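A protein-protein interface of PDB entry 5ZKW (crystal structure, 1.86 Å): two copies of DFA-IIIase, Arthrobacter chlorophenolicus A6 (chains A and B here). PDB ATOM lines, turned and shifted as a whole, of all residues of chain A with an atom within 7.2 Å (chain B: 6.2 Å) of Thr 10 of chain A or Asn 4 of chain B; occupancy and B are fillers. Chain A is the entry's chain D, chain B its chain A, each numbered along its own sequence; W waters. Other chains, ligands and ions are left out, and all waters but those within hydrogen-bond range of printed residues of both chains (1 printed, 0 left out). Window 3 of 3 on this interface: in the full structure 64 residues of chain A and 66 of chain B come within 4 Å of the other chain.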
ATOM      1  N   TYR A   7     -15.228   2.785  19.857  1.00  0.00           N
ATOM      2  CA  TYR A   7     -16.511   3.469  19.895  1.00  0.00           C
ATOM      3  C   TYR A   7     -16.712   4.107  21.261  1.00  0.00           C
ATOM      4  O   TYR A   7     -16.264   3.577  22.284  1.00  0.00           O
ATOM      5  CB  TYR A   7     -17.643   2.483  19.654  1.00  0.00           C
ATOM      6  CG  TYR A   7     -17.618   1.739  18.337  1.00  0.00           C
ATOM      7  CD1 TYR A   7     -16.856   0.599  18.183  1.00  0.00           C
ATOM      8  CD2 TYR A   7     -18.419   2.146  17.260  1.00  0.00           C
ATOM      9  CE1 TYR A   7     -16.859  -0.121  17.001  1.00  0.00           C
ATOM     10  CE2 TYR A   7     -18.427   1.440  16.062  1.00  0.00           C
ATOM     11  CZ  TYR A   7     -17.649   0.302  15.937  1.00  0.00           C
ATOM     12  OH  TYR A   7     -17.630  -0.427  14.770  1.00  0.00           O
ATOM     13  N   ASP A   8     -17.389   5.248  21.260  1.00  0.00           N
ATOM     14  CA  ASP A   8     -17.749   5.963  22.476  1.00  0.00           C
ATOM     15  C   ASP A   8     -19.261   6.132  22.404  1.00  0.00           C
ATOM     16  O   ASP A   8     -19.767   6.710  21.434  1.00  0.00           O
ATOM     17  CB  ASP A   8     -17.006   7.296  22.502  1.00  0.00           C
ATOM     18  CG  ASP A   8     -17.366   8.169  23.688  1.00  0.00           C
ATOM     19  OD1 ASP A   8     -18.519   8.136  24.170  1.00  0.00           O
ATOM     20  OD2 ASP A   8     -16.484   8.935  24.122  1.00  0.00           O
ATOM     21  N   VAL A   9     -19.985   5.626  23.406  1.00  0.00           N
ATOM     22  CA  VAL A   9     -21.455   5.633  23.369  1.00  0.00           C
ATOM     23  C   VAL A   9     -22.081   7.031  23.282  1.00  0.00           C
ATOM     24  O   VAL A   9     -23.230   7.154  22.832  1.00  0.00           O
ATOM     25  CB  VAL A   9     -22.094   4.863  24.556  1.00  0.00           C
ATOM     26  CG1 VAL A   9     -21.687   3.395  24.530  1.00  0.00           C
ATOM     27  CG2 VAL A   9     -21.776   5.512  25.900  1.00  0.00           C
ATOM     28  N   THR A  10     -21.348   8.064  23.719  1.00  0.00           N
ATOM     29  CA  THR A  10     -21.795   9.461  23.622  1.00  0.00           C
ATOM     30  C   THR A  10     -21.456  10.120  22.268  1.00  0.00           C
ATOM     31  O   THR A  10     -21.788  11.281  22.071  1.00  0.00           O
ATOM     32  CB  THR A  10     -21.199  10.354  24.742  1.00  0.00           C
ATOM     33  OG1 THR A  10     -19.783  10.485  24.559  1.00  0.00           O
ATOM     34  CG2 THR A  10     -21.464   9.771  26.123  1.00  0.00           C
ATOM     35  N   GLU A  11     -20.791   9.391  21.369  1.00  0.00           N
ATOM     36  CA  GLU A  11     -20.449   9.872  20.026  1.00  0.00           C
ATOM     37  C   GLU A  11     -20.991   8.894  18.974  1.00  0.00           C
ATOM     38  O   GLU A  11     -20.268   8.462  18.090  1.00  0.00           O
ATOM     39  CB  GLU A  11     -18.930   9.992  19.888  1.00  0.00           C
ATOM     40  CG  GLU A  11     -18.300  11.017  20.826  1.00  0.00           C
ATOM     41  CD  GLU A  11     -16.774  11.039  20.776  1.00  0.00           C
ATOM     42  OE1 GLU A  11     -16.154  10.145  20.149  1.00  0.00           O
ATOM     43  OE2 GLU A  11     -16.186  11.957  21.390  1.00  0.00           O
ATOM     44  N   TRP A  12     -22.259   8.528  19.105  1.00  0.00           N
ATOM     45  CA  TRP A  12     -22.907   7.612  18.174  1.00  0.00           C
ATOM     46  C   TRP A  12     -24.040   8.378  17.521  1.00  0.00           C
ATOM     47  O   TRP A  12     -24.768   9.081  18.212  1.00  0.00           O
ATOM     48  CB  TRP A  12     -23.430   6.382  18.899  1.00  0.00           C
ATOM     49  CG  TRP A  12     -23.828   5.273  17.979  1.00  0.00           C
ATOM     50  CD1 TRP A  12     -25.065   4.730  17.854  1.00  0.00           C
ATOM     51  CD2 TRP A  12     -22.990   4.581  17.046  1.00  0.00           C
ATOM     52  NE1 TRP A  12     -25.059   3.738  16.918  1.00  0.00           N
ATOM     53  CE2 TRP A  12     -23.799   3.619  16.401  1.00  0.00           C
ATOM     54  CE3 TRP A  12     -21.642   4.681  16.689  1.00  0.00           C
ATOM     55  CZ2 TRP A  12     -23.306   2.758  15.426  1.00  0.00           C
ATOM     56  CZ3 TRP A  12     -21.145   3.823  15.717  1.00  0.00           C
ATOM     57  CH2 TRP A  12     -21.980   2.869  15.097  1.00  0.00           C
ATOM     58  N   PRO A  13     -24.177   8.283  16.186  1.00  0.00           N
ATOM     59  CA  PRO A  13     -25.190   9.107  15.493  1.00  0.00           C
ATOM     60  C   PRO A  13     -26.655   8.877  15.877  1.00  0.00           C
ATOM     61  O   PRO A  13     -27.440   9.823  15.822  1.00  0.00           O
ATOM     62  CB  PRO A  13     -24.976   8.751  14.014  1.00  0.00           C
ATOM     63  CG  PRO A  13     -23.551   8.344  13.939  1.00  0.00           C
ATOM     64  CD  PRO A  13     -23.285   7.605  15.221  1.00  0.00           C
ATOM     65  N   PRO A  17     -27.890   7.431  24.509  1.00  0.00           N
ATOM     66  CA  PRO A  17     -27.470   6.508  25.583  1.00  0.00           C
ATOM     67  C   PRO A  17     -28.036   6.850  26.978  1.00  0.00           C
ATOM     68  O   PRO A  17     -28.087   5.967  27.853  1.00  0.00           O
ATOM     69  CB  PRO A  17     -25.942   6.608  25.553  1.00  0.00           C
ATOM     70  CG  PRO A  17     -25.669   7.973  25.038  1.00  0.00           C
ATOM     71  CD  PRO A  17     -26.772   8.281  24.052  1.00  0.00           C
ATOM     72  N   ILE A  21     -29.192   3.052  26.378  1.00  0.00           N
ATOM     73  CA  ILE A  21     -27.834   2.656  25.990  1.00  0.00           C
ATOM     74  C   ILE A  21     -27.791   1.265  25.368  1.00  0.00           C
ATOM     75  O   ILE A  21     -26.904   0.969  24.574  1.00  0.00           O
ATOM     76  CB  ILE A  21     -26.825   2.772  27.163  1.00  0.00           C
ATOM     77  CG1 ILE A  21     -25.377   2.683  26.645  1.00  0.00           C
ATOM     78  CG2 ILE A  21     -27.087   1.723  28.241  1.00  0.00           C
ATOM     79  CD1 ILE A  21     -24.329   3.114  27.651  1.00  0.00           C
ATOM     80  N   VAL A  24     -28.178   1.661  21.657  1.00  0.00           N
ATOM     81  CA  VAL A  24     -26.899   2.232  21.167  1.00  0.00           C
ATOM     82  C   VAL A  24     -25.821   1.147  21.075  1.00  0.00           C
ATOM     83  O   VAL A  24     -25.175   1.005  20.043  1.00  0.00           O
ATOM     84  CB  VAL A  24     -26.422   3.417  22.055  1.00  0.00           C
ATOM     85  CG1 VAL A  24     -25.007   3.879  21.684  1.00  0.00           C
ATOM     86  CG2 VAL A  24     -27.391   4.595  21.953  1.00  0.00           C
ATOM     87  N   ILE A  28     -23.948  -0.480  17.756  1.00  0.00           N
ATOM     88  CA  ILE A  28     -22.494  -0.548  17.612  1.00  0.00           C
ATOM     89  C   ILE A  28     -22.041  -1.963  17.270  1.00  0.00           C
ATOM     90  O   ILE A  28     -21.217  -2.150  16.371  1.00  0.00           O
ATOM     91  CB  ILE A  28     -21.779   0.025  18.870  1.00  0.00           C
ATOM     92  CG1 ILE A  28     -22.005   1.545  18.930  1.00  0.00           C
ATOM     93  CG2 ILE A  28     -20.280  -0.311  18.890  1.00  0.00           C
ATOM     94  CD1 ILE A  28     -21.718   2.185  20.277  1.00  0.00           C
ATOM     95  N   TYR A  52     -16.498   2.351  24.700  1.00  0.00           N
ATOM     96  CA  TYR A  52     -16.208   3.183  25.857  1.00  0.00           C
ATOM     97  C   TYR A  52     -17.458   3.919  26.344  1.00  0.00           C
ATOM     98  O   TYR A  52     -18.207   4.506  25.542  1.00  0.00           O
ATOM     99  CB  TYR A  52     -15.101   4.180  25.525  1.00  0.00           C
ATOM    100  CG  TYR A  52     -14.808   5.127  26.645  1.00  0.00           C
ATOM    101  CD1 TYR A  52     -14.358   4.656  27.871  1.00  0.00           C
ATOM    102  CD2 TYR A  52     -14.991   6.493  26.497  1.00  0.00           C
ATOM    103  CE1 TYR A  52     -14.092   5.519  28.916  1.00  0.00           C
ATOM    104  CE2 TYR A  52     -14.736   7.369  27.533  1.00  0.00           C
ATOM    105  CZ  TYR A  52     -14.289   6.879  28.744  1.00  0.00           C
ATOM    106  OH  TYR A  52     -14.035   7.740  29.764  1.00  0.00           O
ATOM    107  N   LEU A  53     -17.663   3.870  27.660  1.00  0.00           N
ATOM    108  CA  LEU A  53     -18.721   4.588  28.369  1.00  0.00           C
ATOM    109  C   LEU A  53     -18.082   5.664  29.244  1.00  0.00           C
ATOM    110  O   LEU A  53     -17.576   5.354  30.325  1.00  0.00           O
ATOM    111  CB  LEU A  53     -19.496   3.632  29.283  1.00  0.00           C
ATOM    112  CG  LEU A  53     -20.556   2.697  28.692  1.00  0.00           C
ATOM    113  CD1 LEU A  53     -19.963   1.697  27.713  1.00  0.00           C
ATOM    114  CD2 LEU A  53     -21.280   1.965  29.816  1.00  0.00           C
ATOM    115  N   PRO A  54     -18.098   6.931  28.802  1.00  0.00           N
ATOM    116  CA  PRO A  54     -17.630   7.985  29.712  1.00  0.00           C
ATOM    117  C   PRO A  54     -18.502   8.040  30.980  1.00  0.00           C
ATOM    118  O   PRO A  54     -19.597   7.482  30.974  1.00  0.00           O
ATOM    119  CB  PRO A  54     -17.780   9.275  28.898  1.00  0.00           C
ATOM    120  CG  PRO A  54     -18.148   8.893  27.513  1.00  0.00           C
ATOM    121  CD  PRO A  54     -18.611   7.462  27.524  1.00  0.00           C
ATOM    122  N   PRO A  55     -18.020   8.685  32.060  1.00  0.00           N
ATOM    123  CA  PRO A  55     -18.878   8.808  33.241  1.00  0.00           C
ATOM    124  C   PRO A  55     -20.219   9.468  32.875  1.00  0.00           C
ATOM    125  O   PRO A  55     -20.263  10.410  32.070  1.00  0.00           O
ATOM    126  CB  PRO A  55     -18.061   9.685  34.193  1.00  0.00           C
ATOM    127  CG  PRO A  55     -16.630   9.495  33.749  1.00  0.00           C
ATOM    128  CD  PRO A  55     -16.708   9.327  32.264  1.00  0.00           C
ATOM    129  N   GLY A  56     -21.301   8.941  33.432  1.00  0.00           N
ATOM    130  CA  GLY A  56     -22.652   9.390  33.061  1.00  0.00           C
ATOM    131  C   GLY A  56     -23.702   8.412  33.532  1.00  0.00           C
ATOM    132  O   GLY A  56     -23.380   7.279  33.931  1.00  0.00           O
ATOM    133  N   TYR A  58     -26.717   6.271  32.307  1.00  0.00           N
ATOM    134  CA  TYR A  58     -27.242   5.676  31.085  1.00  0.00           C
ATOM    135  C   TYR A  58     -28.333   4.654  31.390  1.00  0.00           C
ATOM    136  O   TYR A  58     -28.056   3.602  31.952  1.00  0.00           O
ATOM    137  CB  TYR A  58     -26.116   4.993  30.311  1.00  0.00           C
ATOM    138  CG  TYR A  58     -24.886   5.839  30.061  1.00  0.00           C
ATOM    139  CD1 TYR A  58     -24.921   6.911  29.175  1.00  0.00           C
ATOM    140  CD2 TYR A  58     -23.681   5.558  30.701  1.00  0.00           C
ATOM    141  CE1 TYR A  58     -23.794   7.685  28.933  1.00  0.00           C
ATOM    142  CE2 TYR A  58     -22.548   6.326  30.471  1.00  0.00           C
ATOM    143  CZ  TYR A  58     -22.599   7.377  29.572  1.00  0.00           C
ATOM    144  OH  TYR A  58     -21.479   8.134  29.325  1.00  0.00           O
ATOM    145  N   PRO B   2     -16.848  19.131  29.784  1.00  0.00           N
ATOM    146  CA  PRO B   2     -17.851  18.985  28.731  1.00  0.00           C
ATOM    147  C   PRO B   2     -18.993  18.068  29.163  1.00  0.00           C
ATOM    148  O   PRO B   2     -18.964  17.509  30.270  1.00  0.00           O
ATOM    149  CB  PRO B   2     -17.059  18.338  27.603  1.00  0.00           C
ATOM    150  CG  PRO B   2     -16.062  17.475  28.315  1.00  0.00           C
ATOM    151  CD  PRO B   2     -15.778  18.128  29.649  1.00  0.00           C
ATOM    152  N   SER B   3     -19.979  17.896  28.287  1.00  0.00           N
ATOM    153  CA  SER B   3     -21.185  17.157  28.650  1.00  0.00           C
ATOM    154  C   SER B   3     -20.930  15.676  28.962  1.00  0.00           C
ATOM    155  O   SER B   3     -21.693  15.088  29.727  1.00  0.00           O
ATOM    156  CB  SER B   3     -22.249  17.282  27.550  1.00  0.00           C
ATOM    157  OG  SER B   3     -21.741  16.779  26.329  1.00  0.00           O
ATOM    158  N   ASN B   4     -19.879  15.070  28.394  1.00  0.00           N
ATOM    159  CA  ASN B   4     -19.593  13.648  28.684  1.00  0.00           C
ATOM    160  C   ASN B   4     -18.626  13.394  29.856  1.00  0.00           C
ATOM    161  O   ASN B   4     -18.147  12.274  30.027  1.00  0.00           O
ATOM    162  CB  ASN B   4     -19.144  12.907  27.430  1.00  0.00           C
ATOM    163  CG  ASN B   4     -17.775  13.315  26.947  1.00  0.00           C
ATOM    164  OD1 ASN B   4     -17.079  14.147  27.546  1.00  0.00           O
ATOM    165  ND2 ASN B   4     -17.374  12.717  25.834  1.00  0.00           N
ATOM    166  N   ASN B   5     -18.322  14.436  30.635  1.00  0.00           N
ATOM    167  CA  ASN B   5     -17.628  14.290  31.919  1.00  0.00           C
ATOM    168  C   ASN B   5     -16.196  13.738  31.797  1.00  0.00           C
ATOM    169  O   ASN B   5     -15.682  13.151  32.747  1.00  0.00           O
ATOM    170  CB  ASN B   5     -18.463  13.427  32.881  1.00  0.00           C
ATOM    171  CG  ASN B   5     -19.862  13.982  33.090  1.00  0.00           C
ATOM    172  OD1 ASN B   5     -20.015  15.159  33.380  1.00  0.00           O
ATOM    173  ND2 ASN B   5     -20.880  13.137  32.945  1.00  0.00           N
ATOM    174  N   ARG B   6     -15.565  13.942  30.639  1.00  0.00           N
ATOM    175  CA  ARG B   6     -14.184  13.517  30.404  1.00  0.00           C
ATOM    176  C   ARG B   6     -13.325  14.766  30.189  1.00  0.00           C
ATOM    177  O   ARG B   6     -13.645  15.610  29.353  1.00  0.00           O
ATOM    178  CB  ARG B   6     -14.117  12.562  29.203  1.00  0.00           C
ATOM    179  CG  ARG B   6     -12.737  11.926  29.027  1.00  0.00           C
ATOM    180  CD  ARG B   6     -12.727  10.649  28.186  1.00  0.00           C
ATOM    181  NE  ARG B   6     -13.318  10.882  26.867  1.00  0.00           N
ATOM    182  CZ  ARG B   6     -12.665  11.317  25.783  1.00  0.00           C
ATOM    183  NH1 ARG B   6     -13.337  11.500  24.649  1.00  0.00           N
ATOM    184  NH2 ARG B   6     -11.355  11.578  25.806  1.00  0.00           N
ATOM    185  N   TYR B   7     -12.262  14.896  30.977  1.00  0.00           N
ATOM    186  CA  TYR B   7     -11.374  16.057  30.950  1.00  0.00           C
ATOM    187  C   TYR B   7      -9.920  15.600  30.783  1.00  0.00           C
ATOM    188  O   TYR B   7      -9.538  14.558  31.286  1.00  0.00           O
ATOM    189  CB  TYR B   7     -11.476  16.847  32.257  1.00  0.00           C
ATOM    190  CG  TYR B   7     -12.841  17.408  32.547  1.00  0.00           C
ATOM    191  CD1 TYR B   7     -13.825  16.631  33.133  1.00  0.00           C
ATOM    192  CD2 TYR B   7     -13.146  18.729  32.231  1.00  0.00           C
ATOM    193  CE1 TYR B   7     -15.083  17.159  33.418  1.00  0.00           C
ATOM    194  CE2 TYR B   7     -14.393  19.261  32.504  1.00  0.00           C
ATOM    195  CZ  TYR B   7     -15.362  18.476  33.096  1.00  0.00           C
ATOM    196  OH  TYR B   7     -16.598  19.029  33.368  1.00  0.00           O
ATOM    197  N   ARG B  35     -21.976  21.769  36.618  1.00  0.00           N
ATOM    198  CA  ARG B  35     -22.833  20.994  35.717  1.00  0.00           C
ATOM    199  C   ARG B  35     -23.663  19.918  36.405  1.00  0.00           C
ATOM    200  O   ARG B  35     -24.721  19.557  35.906  1.00  0.00           O
ATOM    201  CB  ARG B  35     -22.015  20.336  34.596  1.00  0.00           C
ATOM    202  CG  ARG B  35     -21.671  21.248  33.425  1.00  0.00           C
ATOM    203  CD  ARG B  35     -21.051  20.468  32.262  1.00  0.00           C
ATOM    204  NE  ARG B  35     -19.975  19.618  32.765  1.00  0.00           N
ATOM    205  CZ  ARG B  35     -20.064  18.309  33.042  1.00  0.00           C
ATOM    206  NH1 ARG B  35     -21.185  17.618  32.811  1.00  0.00           N
ATOM    207  NH2 ARG B  35     -19.000  17.671  33.542  1.00  0.00           N
ATOM    208  N   VAL B  50     -14.069  11.877  34.868  1.00  0.00           N
ATOM    209  CA  VAL B  50     -12.718  11.360  34.726  1.00  0.00           C
ATOM    210  C   VAL B  50     -11.802  12.482  34.249  1.00  0.00           C
ATOM    211  O   VAL B  50     -12.132  13.221  33.326  1.00  0.00           O
ATOM    212  CB  VAL B  50     -12.662  10.076  33.853  1.00  0.00           C
ATOM    213  CG1 VAL B  50     -13.177  10.303  32.441  1.00  0.00           C
ATOM    214  CG2 VAL B  50     -11.248   9.503  33.828  1.00  0.00           C
HETATM  215  O   HOH W   1     -13.848   8.563  23.347  1.00  0.00           O
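O of Asn 4 of chain B lies close to O of Pro 55 of chain A (3.5 Å). The backbone carbonyl oxygen (O) of Pro 55 of chain A is in hydrogen-bond range of the side-chain amide nitrogen (ND2) of Asn 5 of chain B (2.9 Å).
The backbone carbonyl oxygen (O) of Pro 54 of chain A is in hydrogen-bond range of the side-chain hydroxyl (OH) of Tyr 58 of chain A, 2.6 Å away. The backbone NH (N) of Tyr 7 of chain B is in hydrogen-bond range of the backbone carbonyl oxygen (O) of Val 50 of chain B (2.9 Å). The backbone NH of Val 9 of chain A lies within hydrogen-bond range of the backbone carbonyl oxygen of Tyr 52 of chain A, at 3.0 Å. The backbone NH (N) of Arg 6 of chain B sits close to the side-chain amide oxygen (OD1) of Asn 4 of chain B, at 3.4 Å. The backbone carbonyl oxygen of Tyr 7 of chain A sits at hydrogen-bond distance from the backbone NH of Tyr 52 of chain A (2.7 Å). The backbone carbonyl oxygen of Asn 5 of chain B is in hydrogen-bond range of the backbone NH of Val 50 of chain B (3.0 Å).
Asn 4 of chain B touches Thr 10 of chain A (ND2 to OG1, 3.5 Å). Tyr 52 of chain A touches Arg 6 of chain B (OH to CD, 3.6 Å). Val 50 of chain B touches Tyr 52 of chain A (CG1 to OH, 3.8 Å). Pro 54 of chain A touches Asn 4 of chain B. Pro 55 of chain A touches Val 50 of chain B (CD to CG1, 3.7 Å).
Of chain A, only Thr 10 (3.5 Å), Pro 54 (3.2 Å) and Pro 55 (3.5 Å) come within 4 Å of Asn 4 of chain B. Printed residues of chain A within 4 Å of Asn 5 of chain B: Pro 55 (2.9 Å). Printed residues of chain A within 4 Å of Val 50 of chain B: Tyr 52 (3.8 Å) and Pro 55 (3.7 Å). Printed residues of chain B within 4 Å of Pro 55 of chain A: Asn 4, Asn 5 and Val 50. Printed residues of chain A within 4 Å of Arg 6 of chain B: Tyr 52. Printed residues of chain B within 4 Å of Pro 54 of chain A: Asn 4 (3.2 Å). Ser 3 of chain B touches none of the printed residues of chain A. The nearest printed residue of chain B that does not touch Thr 10 of chain A is Ser 3 of chain B (6.4 Å). The nearest residue of chain A that does not touch Asn 4 of chain B is Asp 8 of chain A (4.2 Å). The nearest printed residue of chain A that does not touch Val 50 of chain B is Pro 54 of chain A (5.7 Å).
Hydrophobic or aromatic side chains of chain A that line the printed part of chain B: Tyr 52, Pro 54 and Pro 55. Of the 8 printed residues of chain B, 4 touch a printed residue of chain A. Among the printed residues, 7 pairs touch across the chains.
Position printed for both chains: 7. Of the 7 pairs that touch across the chains among the printed residues, none has its exchanged pair printed and touching as well.
Water W1 lies within hydrogen-bond range of the side-chain carboxylate (OD2) of Asp 8 of chain A and the guanidinium group (NH1) of Arg 6 of chain B.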
